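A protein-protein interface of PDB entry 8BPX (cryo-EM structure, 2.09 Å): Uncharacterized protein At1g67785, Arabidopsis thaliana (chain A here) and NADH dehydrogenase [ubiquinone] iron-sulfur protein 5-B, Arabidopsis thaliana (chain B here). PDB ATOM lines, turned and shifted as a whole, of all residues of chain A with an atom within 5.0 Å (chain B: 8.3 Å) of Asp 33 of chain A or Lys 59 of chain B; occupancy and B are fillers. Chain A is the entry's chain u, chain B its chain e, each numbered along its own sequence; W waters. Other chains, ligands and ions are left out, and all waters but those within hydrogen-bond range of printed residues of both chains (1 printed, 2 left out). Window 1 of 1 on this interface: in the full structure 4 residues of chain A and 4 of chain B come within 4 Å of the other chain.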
ATOM      1  N   ALA A  29      20.338 -13.509 -20.942  1.00  0.00           N
ATOM      2  CA  ALA A  29      20.918 -13.285 -19.621  1.00  0.00           C
ATOM      3  C   ALA A  29      20.818 -14.533 -18.748  1.00  0.00           C
ATOM      4  O   ALA A  29      21.760 -14.862 -18.016  1.00  0.00           O
ATOM      5  CB  ALA A  29      20.238 -12.100 -18.938  1.00  0.00           C
ATOM      6  N   LEU A  30      19.689 -15.243 -18.811  1.00  0.00           N
ATOM      7  CA  LEU A  30      19.502 -16.408 -17.950  1.00  0.00           C
ATOM      8  C   LEU A  30      20.449 -17.554 -18.283  1.00  0.00           C
ATOM      9  O   LEU A  30      20.640 -18.440 -17.446  1.00  0.00           O
ATOM     10  CB  LEU A  30      18.057 -16.901 -18.022  1.00  0.00           C
ATOM     11  CG  LEU A  30      17.041 -16.096 -17.212  1.00  0.00           C
ATOM     12  CD1 LEU A  30      15.641 -16.283 -17.763  1.00  0.00           C
ATOM     13  CD2 LEU A  30      17.096 -16.483 -15.747  1.00  0.00           C
ATOM     14  N   HIS A  31      21.053 -17.559 -19.470  1.00  0.00           N
ATOM     15  CA  HIS A  31      21.922 -18.646 -19.899  1.00  0.00           C
ATOM     16  C   HIS A  31      23.401 -18.284 -19.848  1.00  0.00           C
ATOM     17  O   HIS A  31      24.215 -18.961 -20.484  1.00  0.00           O
ATOM     18  CB  HIS A  31      21.535 -19.103 -21.306  1.00  0.00           C
ATOM     19  CG  HIS A  31      20.290 -19.932 -21.341  1.00  0.00           C
ATOM     20  ND1 HIS A  31      19.034 -19.400 -21.145  1.00  0.00           N
ATOM     21  CD2 HIS A  31      20.109 -21.260 -21.535  1.00  0.00           C
ATOM     22  CE1 HIS A  31      18.133 -20.363 -21.221  1.00  0.00           C
ATOM     23  NE2 HIS A  31      18.759 -21.502 -21.459  1.00  0.00           N
ATOM     24  N   GLN A  32      23.766 -17.233 -19.111  1.00  0.00           N
ATOM     25  CA  GLN A  32      25.179 -16.889 -18.978  1.00  0.00           C
ATOM     26  C   GLN A  32      25.955 -17.994 -18.269  1.00  0.00           C
ATOM     27  O   GLN A  32      27.072 -18.335 -18.673  1.00  0.00           O
ATOM     28  CB  GLN A  32      25.333 -15.566 -18.226  1.00  0.00           C
ATOM     29  CG  GLN A  32      25.059 -14.324 -19.056  1.00  0.00           C
ATOM     30  CD  GLN A  32      25.772 -14.339 -20.394  1.00  0.00           C
ATOM     31  OE1 GLN A  32      25.157 -14.566 -21.434  1.00  0.00           O
ATOM     32  NE2 GLN A  32      27.076 -14.097 -20.373  1.00  0.00           N
ATOM     33  N   ASP A  33      25.379 -18.561 -17.207  1.00  0.00           N
ATOM     34  CA  ASP A  33      26.097 -19.551 -16.409  1.00  0.00           C
ATOM     35  C   ASP A  33      26.382 -20.820 -17.203  1.00  0.00           C
ATOM     36  O   ASP A  33      27.490 -21.359 -17.139  1.00  0.00           O
ATOM     37  CB  ASP A  33      25.305 -19.876 -15.146  1.00  0.00           C
ATOM     38  CG  ASP A  33      24.625 -18.657 -14.556  1.00  0.00           C
ATOM     39  OD1 ASP A  33      25.290 -17.900 -13.819  1.00  0.00           O
ATOM     40  OD2 ASP A  33      23.422 -18.457 -14.829  1.00  0.00           O
ATOM     41  N   GLU A  34      25.392 -21.319 -17.949  1.00  0.00           N
ATOM     42  CA  GLU A  34      25.609 -22.518 -18.754  1.00  0.00           C
ATOM     43  C   GLU A  34      26.654 -22.276 -19.837  1.00  0.00           C
ATOM     44  O   GLU A  34      27.486 -23.148 -20.110  1.00  0.00           O
ATOM     45  CB  GLU A  34      24.295 -22.986 -19.377  1.00  0.00           C
ATOM     46  CG  GLU A  34      23.355 -23.712 -18.421  1.00  0.00           C
ATOM     47  CD  GLU A  34      22.849 -22.825 -17.298  1.00  0.00           C
ATOM     48  OE1 GLU A  34      21.808 -22.163 -17.483  1.00  0.00           O
ATOM     49  OE2 GLU A  34      23.494 -22.795 -16.228  1.00  0.00           O
ATOM     50  N   LYS A  35      26.615 -21.104 -20.473  1.00  0.00           N
ATOM     51  CA  LYS A  35      27.622 -20.778 -21.476  1.00  0.00           C
ATOM     52  C   LYS A  35      29.011 -20.723 -20.857  1.00  0.00           C
ATOM     53  O   LYS A  35      29.985 -21.202 -21.449  1.00  0.00           O
ATOM     54  CB  LYS A  35      27.281 -19.452 -22.155  1.00  0.00           C
ATOM     55  CG  LYS A  35      28.230 -19.067 -23.271  1.00  0.00           C
ATOM     56  CD  LYS A  35      28.425 -17.560 -23.336  1.00  0.00           C
ATOM     57  CE  LYS A  35      27.174 -16.866 -23.846  1.00  0.00           C
ATOM     58  NZ  LYS A  35      27.415 -16.158 -25.134  1.00  0.00           N
ATOM     59  N   GLN A  36      29.119 -20.150 -19.656  1.00  0.00           N
ATOM     60  CA  GLN A  36      30.398 -20.139 -18.954  1.00  0.00           C
ATOM     61  C   GLN A  36      30.864 -21.554 -18.637  1.00  0.00           C
ATOM     62  O   GLN A  36      32.051 -21.866 -18.769  1.00  0.00           O
ATOM     63  CB  GLN A  36      30.282 -19.317 -17.674  1.00  0.00           C
ATOM     64  CG  GLN A  36      31.000 -17.982 -17.723  1.00  0.00           C
ATOM     65  CD  GLN A  36      31.296 -17.439 -16.341  1.00  0.00           C
ATOM     66  OE1 GLN A  36      31.164 -18.148 -15.344  1.00  0.00           O
ATOM     67  NE2 GLN A  36      31.700 -16.178 -16.273  1.00  0.00           N
ATOM     68  N   GLU A  37      29.944 -22.417 -18.207  1.00  0.00           N
ATOM     69  CA  GLU A  37      30.303 -23.799 -17.902  1.00  0.00           C
ATOM     70  C   GLU A  37      30.804 -24.524 -19.145  1.00  0.00           C
ATOM     71  O   GLU A  37      31.797 -25.259 -19.089  1.00  0.00           O
ATOM     72  CB  GLU A  37      29.100 -24.524 -17.303  1.00  0.00           C
ATOM     73  CG  GLU A  37      29.394 -25.924 -16.795  1.00  0.00           C
ATOM     74  CD  GLU A  37      28.141 -26.647 -16.341  1.00  0.00           C
ATOM     75  OE1 GLU A  37      27.038 -26.085 -16.506  1.00  0.00           O
ATOM     76  OE2 GLU A  37      28.260 -27.773 -15.816  1.00  0.00           O
ATOM     77  N   PHE B  51      26.466  -8.166 -12.210  1.00  0.00           N
ATOM     78  CA  PHE B  51      25.126  -8.488 -12.681  1.00  0.00           C
ATOM     79  C   PHE B  51      24.957  -9.991 -12.873  1.00  0.00           C
ATOM     80  O   PHE B  51      23.880 -10.532 -12.615  1.00  0.00           O
ATOM     81  CB  PHE B  51      24.830  -7.728 -13.976  1.00  0.00           C
ATOM     82  CG  PHE B  51      24.678  -6.240 -13.784  1.00  0.00           C
ATOM     83  CD1 PHE B  51      24.573  -5.700 -12.515  1.00  0.00           C
ATOM     84  CD2 PHE B  51      24.637  -5.383 -14.872  1.00  0.00           C
ATOM     85  CE1 PHE B  51      24.436  -4.342 -12.330  1.00  0.00           C
ATOM     86  CE2 PHE B  51      24.500  -4.019 -14.695  1.00  0.00           C
ATOM     87  CZ  PHE B  51      24.399  -3.497 -13.426  1.00  0.00           C
ATOM     88  N   GLN B  52      26.011 -10.683 -13.311  1.00  0.00           N
ATOM     89  CA  GLN B  52      25.936 -12.135 -13.445  1.00  0.00           C
ATOM     90  C   GLN B  52      25.682 -12.803 -12.096  1.00  0.00           C
ATOM     91  O   GLN B  52      24.844 -13.707 -11.986  1.00  0.00           O
ATOM     92  CB  GLN B  52      27.223 -12.667 -14.068  1.00  0.00           C
ATOM     93  CG  GLN B  52      27.200 -14.152 -14.360  1.00  0.00           C
ATOM     94  CD  GLN B  52      27.924 -14.493 -15.642  1.00  0.00           C
ATOM     95  OE1 GLN B  52      28.512 -13.628 -16.288  1.00  0.00           O
ATOM     96  NE2 GLN B  52      27.868 -15.759 -16.027  1.00  0.00           N
ATOM     97  N   ARG B  53      26.398 -12.370 -11.057  1.00  0.00           N
ATOM     98  CA  ARG B  53      26.209 -12.938  -9.724  1.00  0.00           C
ATOM     99  C   ARG B  53      24.810 -12.642  -9.187  1.00  0.00           C
ATOM    100  O   ARG B  53      24.143 -13.519  -8.615  1.00  0.00           O
ATOM    101  CB  ARG B  53      27.290 -12.395  -8.789  1.00  0.00           C
ATOM    102  CG  ARG B  53      26.938 -12.405  -7.317  1.00  0.00           C
ATOM    103  CD  ARG B  53      28.074 -11.815  -6.501  1.00  0.00           C
ATOM    104  NE  ARG B  53      27.873 -11.998  -5.070  1.00  0.00           N
ATOM    105  CZ  ARG B  53      28.337 -13.031  -4.381  1.00  0.00           C
ATOM    106  NH1 ARG B  53      29.025 -13.997  -4.967  1.00  0.00           N
ATOM    107  NH2 ARG B  53      28.104 -13.095  -3.074  1.00  0.00           N
ATOM    108  N   ARG B  54      24.342 -11.404  -9.367  1.00  0.00           N
ATOM    109  CA  ARG B  54      22.991 -11.077  -8.922  1.00  0.00           C
ATOM    110  C   ARG B  54      21.941 -11.878  -9.686  1.00  0.00           C
ATOM    111  O   ARG B  54      20.916 -12.272  -9.113  1.00  0.00           O
ATOM    112  CB  ARG B  54      22.744  -9.575  -9.055  1.00  0.00           C
ATOM    113  CG  ARG B  54      23.224  -8.796  -7.845  1.00  0.00           C
ATOM    114  CD  ARG B  54      23.615  -7.363  -8.170  1.00  0.00           C
ATOM    115  NE  ARG B  54      22.515  -6.429  -7.971  1.00  0.00           N
ATOM    116  CZ  ARG B  54      22.605  -5.117  -8.140  1.00  0.00           C
ATOM    117  NH1 ARG B  54      23.747  -4.539  -8.475  1.00  0.00           N
ATOM    118  NH2 ARG B  54      21.523  -4.366  -7.968  1.00  0.00           N
ATOM    119  N   ASN B  55      22.187 -12.150 -10.969  1.00  0.00           N
ATOM    120  CA  ASN B  55      21.273 -12.986 -11.735  1.00  0.00           C
ATOM    121  C   ASN B  55      21.299 -14.426 -11.249  1.00  0.00           C
ATOM    122  O   ASN B  55      20.274 -15.104 -11.292  1.00  0.00           O
ATOM    123  CB  ASN B  55      21.610 -12.917 -13.222  1.00  0.00           C
ATOM    124  CG  ASN B  55      21.267 -11.571 -13.835  1.00  0.00           C
ATOM    125  OD1 ASN B  55      20.545 -10.773 -13.240  1.00  0.00           O
ATOM    126  ND2 ASN B  55      21.780 -11.318 -15.030  1.00  0.00           N
ATOM    127  N   ARG B  56      22.458 -14.909 -10.801  1.00  0.00           N
ATOM    128  CA  ARG B  56      22.504 -16.221 -10.160  1.00  0.00           C
ATOM    129  C   ARG B  56      21.623 -16.251  -8.917  1.00  0.00           C
ATOM    130  O   ARG B  56      20.908 -17.232  -8.671  1.00  0.00           O
ATOM    131  CB  ARG B  56      23.943 -16.586  -9.800  1.00  0.00           C
ATOM    132  CG  ARG B  56      24.559 -17.610 -10.714  1.00  0.00           C
ATOM    133  CD  ARG B  56      25.991 -17.906 -10.337  1.00  0.00           C
ATOM    134  NE  ARG B  56      26.897 -17.744 -11.466  1.00  0.00           N
ATOM    135  CZ  ARG B  56      27.687 -16.696 -11.646  1.00  0.00           C
ATOM    136  NH1 ARG B  56      27.721 -15.700 -10.777  1.00  0.00           N
ATOM    137  NH2 ARG B  56      28.469 -16.650 -12.720  1.00  0.00           N
ATOM    138  N   ILE B  57      21.665 -15.181  -8.122  1.00  0.00           N
ATOM    139  CA  ILE B  57      20.817 -15.118  -6.931  1.00  0.00           C
ATOM    140  C   ILE B  57      19.343 -15.161  -7.326  1.00  0.00           C
ATOM    141  O   ILE B  57      18.540 -15.903  -6.742  1.00  0.00           O
ATOM    142  CB  ILE B  57      21.140 -13.863  -6.102  1.00  0.00           C
ATOM    143  CG1 ILE B  57      22.483 -14.021  -5.393  1.00  0.00           C
ATOM    144  CG2 ILE B  57      20.038 -13.590  -5.083  1.00  0.00           C
ATOM    145  CD1 ILE B  57      23.110 -12.710  -5.000  1.00  0.00           C
ATOM    146  N   TYR B  58      18.972 -14.371  -8.335  1.00  0.00           N
ATOM    147  CA  TYR B  58      17.590 -14.369  -8.816  1.00  0.00           C
ATOM    148  C   TYR B  58      17.188 -15.739  -9.357  1.00  0.00           C
ATOM    149  O   TYR B  58      16.052 -16.189  -9.158  1.00  0.00           O
ATOM    150  CB  TYR B  58      17.417 -13.289  -9.883  1.00  0.00           C
ATOM    151  CG  TYR B  58      16.254 -13.505 -10.828  1.00  0.00           C
ATOM    152  CD1 TYR B  58      14.967 -13.125 -10.477  1.00  0.00           C
ATOM    153  CD2 TYR B  58      16.449 -14.081 -12.076  1.00  0.00           C
ATOM    154  CE1 TYR B  58      13.907 -13.318 -11.340  1.00  0.00           C
ATOM    155  CE2 TYR B  58      15.393 -14.279 -12.943  1.00  0.00           C
ATOM    156  CZ  TYR B  58      14.129 -13.897 -12.573  1.00  0.00           C
ATOM    157  OH  TYR B  58      13.079 -14.094 -13.440  1.00  0.00           O
ATOM    158  N   LYS B  59      18.107 -16.407 -10.054  1.00  0.00           N
ATOM    159  CA  LYS B  59      17.854 -17.739 -10.591  1.00  0.00           C
ATOM    160  C   LYS B  59      17.559 -18.730  -9.477  1.00  0.00           C
ATOM    161  O   LYS B  59      16.606 -19.512  -9.560  1.00  0.00           O
ATOM    162  CB  LYS B  59      19.067 -18.202 -11.397  1.00  0.00           C
ATOM    163  CG  LYS B  59      18.804 -19.322 -12.375  1.00  0.00           C
ATOM    164  CD  LYS B  59      19.769 -19.250 -13.549  1.00  0.00           C
ATOM    165  CE  LYS B  59      20.156 -17.816 -13.875  1.00  0.00           C
ATOM    166  NZ  LYS B  59      20.862 -17.725 -15.179  1.00  0.00           N
ATOM    167  N   GLU B  60      18.384 -18.725  -8.430  1.00  0.00           N
ATOM    168  CA  GLU B  60      18.158 -19.638  -7.315  1.00  0.00           C
ATOM    169  C   GLU B  60      16.845 -19.324  -6.609  1.00  0.00           C
ATOM    170  O   GLU B  60      16.136 -20.234  -6.159  1.00  0.00           O
ATOM    171  CB  GLU B  60      19.334 -19.579  -6.342  1.00  0.00           C
ATOM    172  CG  GLU B  60      19.202 -20.528  -5.167  1.00  0.00           C
ATOM    173  CD  GLU B  60      19.609 -21.943  -5.524  1.00  0.00           C
ATOM    174  OE1 GLU B  60      20.576 -22.111  -6.297  1.00  0.00           O
ATOM    175  OE2 GLU B  60      18.961 -22.890  -5.031  1.00  0.00           O
ATOM    176  N   GLU B  61      16.496 -18.038  -6.513  1.00  0.00           N
ATOM    177  CA  GLU B  61      15.202 -17.679  -5.943  1.00  0.00           C
ATOM    178  C   GLU B  61      14.056 -18.236  -6.776  1.00  0.00           C
ATOM    179  O   GLU B  61      13.068 -18.740  -6.230  1.00  0.00           O
ATOM    180  CB  GLU B  61      15.077 -16.161  -5.816  1.00  0.00           C
ATOM    181  CG  GLU B  61      14.057 -15.722  -4.787  1.00  0.00           C
ATOM    182  CD  GLU B  61      13.660 -14.268  -4.940  1.00  0.00           C
ATOM    183  OE1 GLU B  61      13.909 -13.691  -6.020  1.00  0.00           O
ATOM    184  OE2 GLU B  61      13.097 -13.701  -3.981  1.00  0.00           O
ATOM    185  N   GLN B  62      14.168 -18.157  -8.103  1.00  0.00           N
ATOM    186  CA  GLN B  62      13.110 -18.688  -8.958  1.00  0.00           C
ATOM    187  C   GLN B  62      13.071 -20.211  -8.924  1.00  0.00           C
ATOM    188  O   GLN B  62      12.013 -20.810  -9.144  1.00  0.00           O
ATOM    189  CB  GLN B  62      13.292 -18.194 -10.393  1.00  0.00           C
ATOM    190  CG  GLN B  62      12.035 -17.627 -11.041  1.00  0.00           C
ATOM    191  CD  GLN B  62      11.440 -16.457 -10.272  1.00  0.00           C
ATOM    192  OE1 GLN B  62      12.133 -15.771  -9.521  1.00  0.00           O
ATOM    193  NE2 GLN B  62      10.147 -16.225 -10.461  1.00  0.00           N
ATOM    194  N   ARG B  63      14.213 -20.849  -8.666  1.00  0.00           N
ATOM    195  CA  ARG B  63      14.253 -22.305  -8.590  1.00  0.00           C
ATOM    196  C   ARG B  63      13.631 -22.814  -7.294  1.00  0.00           C
ATOM    197  O   ARG B  63      12.937 -23.837  -7.295  1.00  0.00           O
ATOM    198  CB  ARG B  63      15.694 -22.794  -8.723  1.00  0.00           C
ATOM    199  CG  ARG B  63      15.828 -24.284  -8.895  1.00  0.00           C
ATOM    200  CD  ARG B  63      17.250 -24.744  -8.629  1.00  0.00           C
ATOM    201  NE  ARG B  63      17.635 -24.571  -7.235  1.00  0.00           N
ATOM    202  CZ  ARG B  63      17.326 -25.416  -6.262  1.00  0.00           C
ATOM    203  NH1 ARG B  63      16.607 -26.504  -6.495  1.00  0.00           N
ATOM    204  NH2 ARG B  63      17.750 -25.169  -5.027  1.00  0.00           N
ATOM    205  N   LYS B  64      13.861 -22.114  -6.180  1.00  0.00           N
ATOM    206  CA  LYS B  64      13.335 -22.533  -4.883  1.00  0.00           C
ATOM    207  C   LYS B  64      11.951 -21.965  -4.592  1.00  0.00           C
ATOM    208  O   LYS B  64      11.597 -21.781  -3.418  1.00  0.00           O
ATOM    209  CB  LYS B  64      14.303 -22.145  -3.766  1.00  0.00           C
ATOM    210  CG  LYS B  64      15.620 -22.884  -3.782  1.00  0.00           C
ATOM    211  CD  LYS B  64      16.466 -22.496  -2.580  1.00  0.00           C
ATOM    212  CE  LYS B  64      17.308 -23.664  -2.091  1.00  0.00           C
ATOM    213  NZ  LYS B  64      17.684 -23.512  -0.660  1.00  0.00           N
ATOM    214  N   LEU B  65      11.156 -21.679  -5.617  1.00  0.00           N
ATOM    215  CA  LEU B  65       9.826 -21.118  -5.410  1.00  0.00           C
ATOM    216  C   LEU B  65       8.807 -21.722  -6.370  1.00  0.00           C
ATOM    217  O   LEU B  65       9.004 -21.719  -7.583  1.00  0.00           O
ATOM    218  CB  LEU B  65       9.856 -19.597  -5.572  1.00  0.00           C
ATOM    219  CG  LEU B  65       8.501 -18.889  -5.560  1.00  0.00           C
ATOM    220  CD1 LEU B  65       7.801 -19.079  -4.222  1.00  0.00           C
ATOM    221  CD2 LEU B  65       8.660 -17.411  -5.884  1.00  0.00           C
HETATM  222  O   HOH W   1      23.325 -13.521 -16.088  1.00  0.00           O
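The side-chain amino group of Lys 59 of chain B sits close to the backbone carbonyl oxygen of Leu 30 of chain A. The side-chain carboxylate of Asp 33 of chain A is in salt-bridge range of the side-chain amino group of Lys 59 of chain B (2.7 Å). The guanidinium group (NE) of Arg 56 of chain B is in salt-bridge range of the side-chain carboxylate (OD1) of Asp 33 of chain A (2.9 Å).
Water W1 bridges the backbone carbonyl oxygen of Ala 29 of chain A (2.8 Å) and the side-chain amide nitrogen of Asn 55 of chain B (2.9 Å).
Printed residues of chain A that touch a printed residue of chain B: Leu 30, Gln 32, Asp 33 and Gln 36. Hydrophobic or aromatic side chains of chain A within 4 Å of the printed part of chain B: Leu 30. Printed residues of chain B that touch a printed residue of chain A: Gln 52, Arg 56, Tyr 58 and Lys 59. Among the printed residues, Asp or Glu carboxylates within 4 Å of a Lys or Arg side-chain nitrogen of the other chain: Asp 33 of chain A with Arg 56 of chain B (2.9 Å) and Asp 33 of chain A with Lys 59 of chain B (2.7 Å).
Among the printed residues, merely in contact across the chains: Gln 32 of chain A with Gln 52 of chain B (3.4 Å), Gln 36 of chain A with Gln 52 of chain B (3.8 Å), Asp 33 of chain A with Gln 52 of chain B (3.9 Å) and Leu 30 of chain A with Tyr 58 of chain B (3.95 Å).
Of the printed residues of chain B, Leu 30 of chain A touches Tyr 58 (3.95 Å) and Lys 59 (2.4 Å). Of the printed residues of chain B, Gln 32 of chain A touches Gln 52 (3.4 Å). Asp 33 of chain A touches just these residues of chain B: Gln 52 (3.9 Å), Arg 56 (2.9 Å) and Lys 59 (2.7 Å). Printed residues of chain B within 4 Å of Gln 36 of chain A: Gln 52. Printed residues of chain A within 4 Å of Gln 52 of chain B: Gln 32 (3.4 Å), Asp 33 (3.9 Å) and Gln 36 (3.8 Å). Of the printed residues of chain A, Tyr 58 of chain B touches Leu 30 (3.95 Å). Arg 63 of chain B touches none of the printed residues of chain A. The nearest residue of chain B that does not touch Asp 33 of chain A is Asn 55 of chain B (5.8 Å).
NE2 of Gln 52 of chain B lies close to NH2 of Arg 56 of chain B, at 3.5 Å.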
